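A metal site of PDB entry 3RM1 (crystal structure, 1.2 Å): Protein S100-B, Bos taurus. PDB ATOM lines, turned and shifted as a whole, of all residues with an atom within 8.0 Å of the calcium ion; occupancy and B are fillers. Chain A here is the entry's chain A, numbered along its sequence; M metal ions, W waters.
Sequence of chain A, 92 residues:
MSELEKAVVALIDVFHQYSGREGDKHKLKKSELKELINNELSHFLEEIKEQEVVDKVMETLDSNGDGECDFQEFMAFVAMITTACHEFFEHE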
ATOM      1  N   PHE A  15      -2.407  33.946   0.719  1.00  0.00           N
ATOM      2  CA  PHE A  15      -3.154  32.719   0.433  1.00  0.00           C
ATOM      3  C   PHE A  15      -2.305  31.517   0.763  1.00  0.00           C
ATOM      4  O   PHE A  15      -2.769  30.603   1.467  1.00  0.00           O
ATOM      5  CB  PHE A  15      -3.632  32.647  -1.026  1.00  0.00           C
ATOM      6  CG  PHE A  15      -4.290  31.329  -1.373  1.00  0.00           C
ATOM      7  CD1 PHE A  15      -5.642  31.117  -1.083  1.00  0.00           C
ATOM      8  CD2 PHE A  15      -3.565  30.317  -1.984  1.00  0.00           C
ATOM      9  CE1 PHE A  15      -6.244  29.942  -1.388  1.00  0.00           C
ATOM     10  CE2 PHE A  15      -4.183  29.104  -2.309  1.00  0.00           C
ATOM     11  CZ  PHE A  15      -5.522  28.919  -1.984  1.00  0.00           C
ATOM     12  N   HIS A  16      -1.087  31.501   0.265  1.00  0.00           N
ATOM     13  CA  HIS A  16      -0.235  30.349   0.444  1.00  0.00           C
ATOM     14  C   HIS A  16       0.294  30.183   1.878  1.00  0.00           C
ATOM     15  O   HIS A  16       0.514  29.033   2.303  1.00  0.00           O
ATOM     16  CB  HIS A  16       0.835  30.405  -0.608  1.00  0.00           C
ATOM     17  CG  HIS A  16       0.335  29.978  -1.955  1.00  0.00           C
ATOM     18  ND1 HIS A  16      -0.038  30.870  -2.951  1.00  0.00           N
ATOM     19  CD2 HIS A  16       0.121  28.736  -2.454  1.00  0.00           C
ATOM     20  CE1 HIS A  16      -0.425  30.182  -4.012  1.00  0.00           C
ATOM     21  NE2 HIS A  16      -0.347  28.903  -3.736  1.00  0.00           N
ATOM     22  N   GLN A  17       0.452  31.267   2.628  1.00  0.00           N
ATOM     23  CA  GLN A  17       0.784  31.179   4.052  1.00  0.00           C
ATOM     24  C   GLN A  17      -0.272  30.285   4.748  1.00  0.00           C
ATOM     25  O   GLN A  17       0.066  29.385   5.543  1.00  0.00           O
ATOM     26  CB  GLN A  17       0.793  32.557   4.733  1.00  0.00           C
ATOM     27  CG  GLN A  17       2.039  33.420   4.532  1.00  0.00           C
ATOM     28  CD  GLN A  17       1.799  34.909   4.828  1.00  0.00           C
ATOM     29  OE1 GLN A  17       0.762  35.291   5.392  1.00  0.00           O
ATOM     30  NE2 GLN A  17       2.744  35.756   4.414  1.00  0.00           N
ATOM     31  N   TYR A  18      -1.538  30.485   4.440  1.00  0.00           N
ATOM     32  CA  TYR A  18      -2.605  29.746   5.083  1.00  0.00           C
ATOM     33  C   TYR A  18      -2.901  28.432   4.413  1.00  0.00           C
ATOM     34  O   TYR A  18      -3.117  27.429   5.105  1.00  0.00           O
ATOM     35  CB  TYR A  18      -3.858  30.626   5.224  1.00  0.00           C
ATOM     36  CG  TYR A  18      -3.667  31.663   6.310  1.00  0.00           C
ATOM     37  CD1 TYR A  18      -3.045  32.884   6.063  1.00  0.00           C
ATOM     38  CD2 TYR A  18      -4.045  31.351   7.610  1.00  0.00           C
ATOM     39  CE1 TYR A  18      -2.819  33.801   7.095  1.00  0.00           C
ATOM     40  CE2 TYR A  18      -3.813  32.251   8.630  1.00  0.00           C
ATOM     41  CZ  TYR A  18      -3.186  33.459   8.388  1.00  0.00           C
ATOM     42  OH  TYR A  18      -2.983  34.327   9.440  1.00  0.00           O
ATOM     43  N   SER A  19      -2.868  28.386   3.093  1.00  0.00           N
ATOM     44  CA  SER A  19      -3.223  27.150   2.393  1.00  0.00           C
ATOM     45  C   SER A  19      -2.193  26.044   2.630  1.00  0.00           C
ATOM     46  O   SER A  19      -2.544  24.854   2.617  1.00  0.00           O
ATOM     47  CB  SER A  19      -3.432  27.353   0.902  1.00  0.00           C
ATOM     48  OG  SER A  19      -2.256  27.689   0.227  1.00  0.00           O
ATOM     49  N   GLY A  20      -0.948  26.425   2.831  1.00  0.00           N
ATOM     50  CA  GLY A  20       0.134  25.460   3.018  1.00  0.00           C
ATOM     51  C   GLY A  20       0.219  24.873   4.416  1.00  0.00           C
ATOM     52  O   GLY A  20       1.123  24.085   4.670  1.00  0.00           O
ATOM     53  N   ARG A  21      -0.656  25.267   5.336  1.00  0.00           N
ATOM     54  CA  ARG A  21      -0.559  24.732   6.686  1.00  0.00           C
ATOM     55  C   ARG A  21      -0.821  23.231   6.804  1.00  0.00           C
ATOM     56  O   ARG A  21      -0.065  22.509   7.465  1.00  0.00           O
ATOM     57  CB  ARG A  21      -1.481  25.509   7.625  1.00  0.00           C
ATOM     58  CG  ARG A  21      -1.047  26.934   7.852  1.00  0.00           C
ATOM     59  CD  ARG A  21      -2.029  27.674   8.714  1.00  0.00           C
ATOM     60  NE  ARG A  21      -1.518  28.973   9.129  1.00  0.00           N
ATOM     61  CZ  ARG A  21      -2.022  29.698  10.118  1.00  0.00           C
ATOM     62  NH1 ARG A  21      -3.089  29.260  10.793  1.00  0.00           N
ATOM     63  NH2 ARG A  21      -1.465  30.848  10.471  1.00  0.00           N
ATOM     64  N   GLU A  22      -1.894  22.751   6.191  1.00  0.00           N
ATOM     65  CA  GLU A  22      -2.387  21.398   6.418  1.00  0.00           C
ATOM     66  C   GLU A  22      -2.978  20.875   5.134  1.00  0.00           C
ATOM     67  O   GLU A  22      -3.468  21.650   4.279  1.00  0.00           O
ATOM     68  CB  GLU A  22      -3.468  21.394   7.495  1.00  0.00           C
ATOM     69  CG  GLU A  22      -2.999  21.743   8.903  1.00  0.00           C
ATOM     70  CD  GLU A  22      -4.145  21.784   9.911  1.00  0.00           C
ATOM     71  OE1 GLU A  22      -5.130  21.025   9.778  1.00  0.00           O
ATOM     72  OE2 GLU A  22      -4.045  22.597  10.864  1.00  0.00           O
ATOM     73  N   GLY A  23      -2.936  19.547   4.990  1.00  0.00           N
ATOM     74  CA  GLY A  23      -3.530  18.863   3.864  1.00  0.00           C
ATOM     75  C   GLY A  23      -3.042  19.384   2.525  1.00  0.00           C
ATOM     76  O   GLY A  23      -1.859  19.638   2.318  1.00  0.00           O
ATOM     77  N   ASP A  24      -3.983  19.536   1.597  1.00  0.00           N
ATOM     78  CA  ASP A  24      -3.680  20.107   0.295  1.00  0.00           C
ATOM     79  C   ASP A  24      -3.002  21.473   0.468  1.00  0.00           C
ATOM     80  O   ASP A  24      -3.587  22.392   1.066  1.00  0.00           O
ATOM     81  CB  ASP A  24      -4.981  20.282  -0.478  1.00  0.00           C
ATOM     82  CG  ASP A  24      -4.761  20.606  -1.941  1.00  0.00           C
ATOM     83  OD1 ASP A  24      -3.862  21.365  -2.303  1.00  0.00           O
ATOM     84  OD2 ASP A  24      -5.475  20.035  -2.783  1.00  0.00           O
ATOM     85  N   LYS A  25      -1.800  21.640  -0.063  1.00  0.00           N
ATOM     86  CA  LYS A  25      -1.065  22.906   0.124  1.00  0.00           C
ATOM     87  C   LYS A  25      -1.550  24.025  -0.769  1.00  0.00           C
ATOM     88  O   LYS A  25      -1.132  25.167  -0.588  1.00  0.00           O
ATOM     89  CB  LYS A  25       0.433  22.683  -0.039  1.00  0.00           C
ATOM     90  CG  LYS A  25       0.997  21.794   1.038  1.00  0.00           C
ATOM     91  N   HIS A  26      -2.441  23.717  -1.708  1.00  0.00           N
ATOM     92  CA  HIS A  26      -2.908  24.723  -2.640  1.00  0.00           C
ATOM     93  C   HIS A  26      -4.320  25.148  -2.375  1.00  0.00           C
ATOM     94  O   HIS A  26      -4.907  25.916  -3.143  1.00  0.00           O
ATOM     95  CB  HIS A  26      -2.744  24.233  -4.081  1.00  0.00           C
ATOM     96  CG  HIS A  26      -1.319  24.201  -4.522  1.00  0.00           C
ATOM     97  ND1 HIS A  26      -0.523  23.086  -4.378  1.00  0.00           N
ATOM     98  CD2 HIS A  26      -0.525  25.163  -5.047  1.00  0.00           C
ATOM     99  CE1 HIS A  26       0.683  23.355  -4.833  1.00  0.00           C
ATOM    100  NE2 HIS A  26       0.718  24.606  -5.243  1.00  0.00           N
ATOM    101  N   LYS A  27      -4.894  24.622  -1.285  1.00  0.00           N
ATOM    102  CA  LYS A  27      -6.259  24.962  -0.908  1.00  0.00           C
ATOM    103  C   LYS A  27      -6.383  25.220   0.560  1.00  0.00           C
ATOM    104  O   LYS A  27      -5.611  24.638   1.364  1.00  0.00           O
ATOM    105  CB  LYS A  27      -7.265  23.876  -1.335  1.00  0.00           C
ATOM    106  CG  LYS A  27      -7.226  23.553  -2.818  1.00  0.00           C
ATOM    107  CD  LYS A  27      -8.241  22.448  -3.134  1.00  0.00           C
ATOM    108  CE  LYS A  27      -8.123  21.893  -4.569  1.00  0.00           C
ATOM    109  NZ  LYS A  27      -8.981  20.659  -4.708  1.00  0.00           N
ATOM    110  N   LEU A  28      -7.345  26.076   0.883  1.00  0.00           N
ATOM    111  CA  LEU A  28      -7.748  26.371   2.257  1.00  0.00           C
ATOM    112  C   LEU A  28      -8.853  25.443   2.716  1.00  0.00           C
ATOM    113  O   LEU A  28      -9.950  25.453   2.168  1.00  0.00           O
ATOM    114  CB  LEU A  28      -8.292  27.780   2.367  1.00  0.00           C
ATOM    115  CG  LEU A  28      -7.368  28.921   1.963  1.00  0.00           C
ATOM    116  CD1 LEU A  28      -8.130  30.231   1.742  1.00  0.00           C
ATOM    117  CD2 LEU A  28      -6.227  29.172   2.976  1.00  0.00           C
ATOM    118  N   LYS A  29      -8.586  24.622   3.718  1.00  0.00           N
ATOM    119  CA  LYS A  29      -9.650  23.910   4.431  1.00  0.00           C
ATOM    120  C   LYS A  29     -10.337  24.878   5.409  1.00  0.00           C
ATOM    121  O   LYS A  29      -9.880  26.004   5.610  1.00  0.00           O
ATOM    122  CB  LYS A  29      -9.141  22.647   5.148  1.00  0.00           C
ATOM    123  CG  LYS A  29      -8.141  22.938   6.248  1.00  0.00           C
ATOM    124  CD  LYS A  29      -7.486  21.632   6.776  1.00  0.00           C
ATOM    125  CE  LYS A  29      -8.383  20.876   7.731  1.00  0.00           C
ATOM    126  N   LYS A  30     -11.396  24.429   6.064  1.00  0.00           N
ATOM    127  CA  LYS A  30     -12.147  25.320   6.947  1.00  0.00           C
ATOM    128  C   LYS A  30     -11.290  26.014   7.984  1.00  0.00           C
ATOM    129  O   LYS A  30     -11.416  27.230   8.180  1.00  0.00           O
ATOM    130  CB  LYS A  30     -13.261  24.545   7.654  1.00  0.00           C
ATOM    131  CG  LYS A  30     -14.470  24.275   6.776  1.00  0.00           C
ATOM    132  CD  LYS A  30     -15.472  23.397   7.520  1.00  0.00           C
ATOM    133  CE  LYS A  30     -16.680  23.062   6.683  1.00  0.00           C
ATOM    134  NZ  LYS A  30     -17.563  22.186   7.453  1.00  0.00           N
ATOM    135  N   SER A  31     -10.432  25.273   8.678  1.00  0.00           N
ATOM    136  CA  SER A  31      -9.635  25.880   9.765  1.00  0.00           C
ATOM    137  C   SER A  31      -8.654  26.919   9.198  1.00  0.00           C
ATOM    138  O   SER A  31      -8.450  27.966   9.817  1.00  0.00           O
ATOM    139  CB  SER A  31      -8.889  24.796  10.549  1.00  0.00           C
ATOM    140  OG  SER A  31      -7.997  24.101   9.714  1.00  0.00           O
ATOM    141  N   GLU A  32      -8.078  26.650   8.029  1.00  0.00           N
ATOM    142  CA  GLU A  32      -7.119  27.588   7.409  1.00  0.00           C
ATOM    143  C   GLU A  32      -7.850  28.831   6.970  1.00  0.00           C
ATOM    144  O   GLU A  32      -7.359  29.952   7.187  1.00  0.00           O
ATOM    145  CB  GLU A  32      -6.450  26.936   6.194  1.00  0.00           C
ATOM    146  CG  GLU A  32      -5.502  25.814   6.566  1.00  0.00           C
ATOM    147  CD  GLU A  32      -5.054  25.021   5.364  1.00  0.00           C
ATOM    148  OE1 GLU A  32      -5.807  24.947   4.362  1.00  0.00           O
ATOM    149  OE2 GLU A  32      -3.968  24.396   5.400  1.00  0.00           O
ATOM    150  N   LEU A  33      -9.053  28.674   6.415  1.00  0.00           N
ATOM    151  CA  LEU A  33      -9.858  29.820   6.015  1.00  0.00           C
ATOM    152  C   LEU A  33     -10.271  30.668   7.213  1.00  0.00           C
ATOM    153  O   LEU A  33     -10.212  31.919   7.146  1.00  0.00           O
ATOM    154  CB  LEU A  33     -11.063  29.356   5.198  1.00  0.00           C
ATOM    155  CG  LEU A  33     -12.081  30.408   4.735  1.00  0.00           C
ATOM    156  CD1 LEU A  33     -11.482  31.451   3.814  1.00  0.00           C
ATOM    157  CD2 LEU A  33     -13.266  29.693   4.090  1.00  0.00           C
ATOM    158  N   GLU A  68     -13.084  22.787  -0.134  1.00  0.00           N
ATOM    159  CA  GLU A  68     -11.967  23.676   0.184  1.00  0.00           C
ATOM    160  C   GLU A  68     -12.033  24.905  -0.679  1.00  0.00           C
ATOM    161  O   GLU A  68     -12.731  24.913  -1.698  1.00  0.00           O
ATOM    162  CB  GLU A  68     -10.609  22.976   0.020  1.00  0.00           C
ATOM    163  CG  GLU A  68     -10.486  21.717   0.909  1.00  0.00           C
ATOM    164  CD  GLU A  68      -9.070  21.373   1.320  1.00  0.00           C
ATOM    165  OE1 GLU A  68      -8.217  22.256   1.364  1.00  0.00           O
ATOM    166  OE2 GLU A  68      -8.835  20.206   1.660  1.00  0.00           O
ATOM    167  N   CYS A  69     -11.301  25.951  -0.277  1.00  0.00           N
ATOM    168  CA  CYS A  69     -11.247  27.174  -1.067  1.00  0.00           C
ATOM    169  C   CYS A  69      -9.906  27.224  -1.805  1.00  0.00           C
ATOM    170  O   CYS A  69      -8.844  27.361  -1.168  1.00  0.00           O
ATOM    171  CB  CYS A  69     -11.383  28.378  -0.129  1.00  0.00           C
ATOM    172  SG  CYS A  69     -11.397  29.984  -0.969  1.00  0.00           S
HETATM  173 CA    CA M   1      -4.406  23.451   3.024  1.00  0.00          CA
HETATM  174  O   HOH W   1      -6.225  22.041   3.057  1.00  0.00           O
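Five residues have an atom within 4 Å of the calcium ion: Ser 19, Glu 22, Asp 24, Lys 27 and Glu 32.
Along chain A the residues within 4 Å of the calcium ion span positions 19 to 32.
The calcium ion is bound by water W1 (2.3 Å).
O of Ser 19 is bound to the calcium ion (2.4 Å).
O of Lys 27 is bound to the calcium ion (2.4 Å).
O of Asp 24 binds the calcium ion (2.4 Å).
The backbone carbonyl oxygen (O) of Glu 22 binds the calcium ion.
The side-chain carboxylate (OE1) of Glu 32 binds the calcium ion, 2.4 Å away.
OE2 of Glu 32 is bound to the calcium ion, 2.6 Å away.
The calcium ion has seven donor atoms within binding distance.
The side-chain hydroxyl of Ser 19 lies within hydrogen-bond range of the backbone carbonyl oxygen of Lys 25.
The side-chain hydroxyl (OG) of Ser 19 lies within hydrogen-bond range of the backbone carbonyl oxygen (O) of Phe 15, at 3.2 Å.
OD1 of Asp 24 lies within hydrogen-bond range of N of His 26 (2.8 Å).
OE1 of Glu 32 lies close to N of Lys 29 (2.9 Å).
The side-chain carboxylate of Glu 32 sits close to the backbone NH of Arg 21 (3.4 Å).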
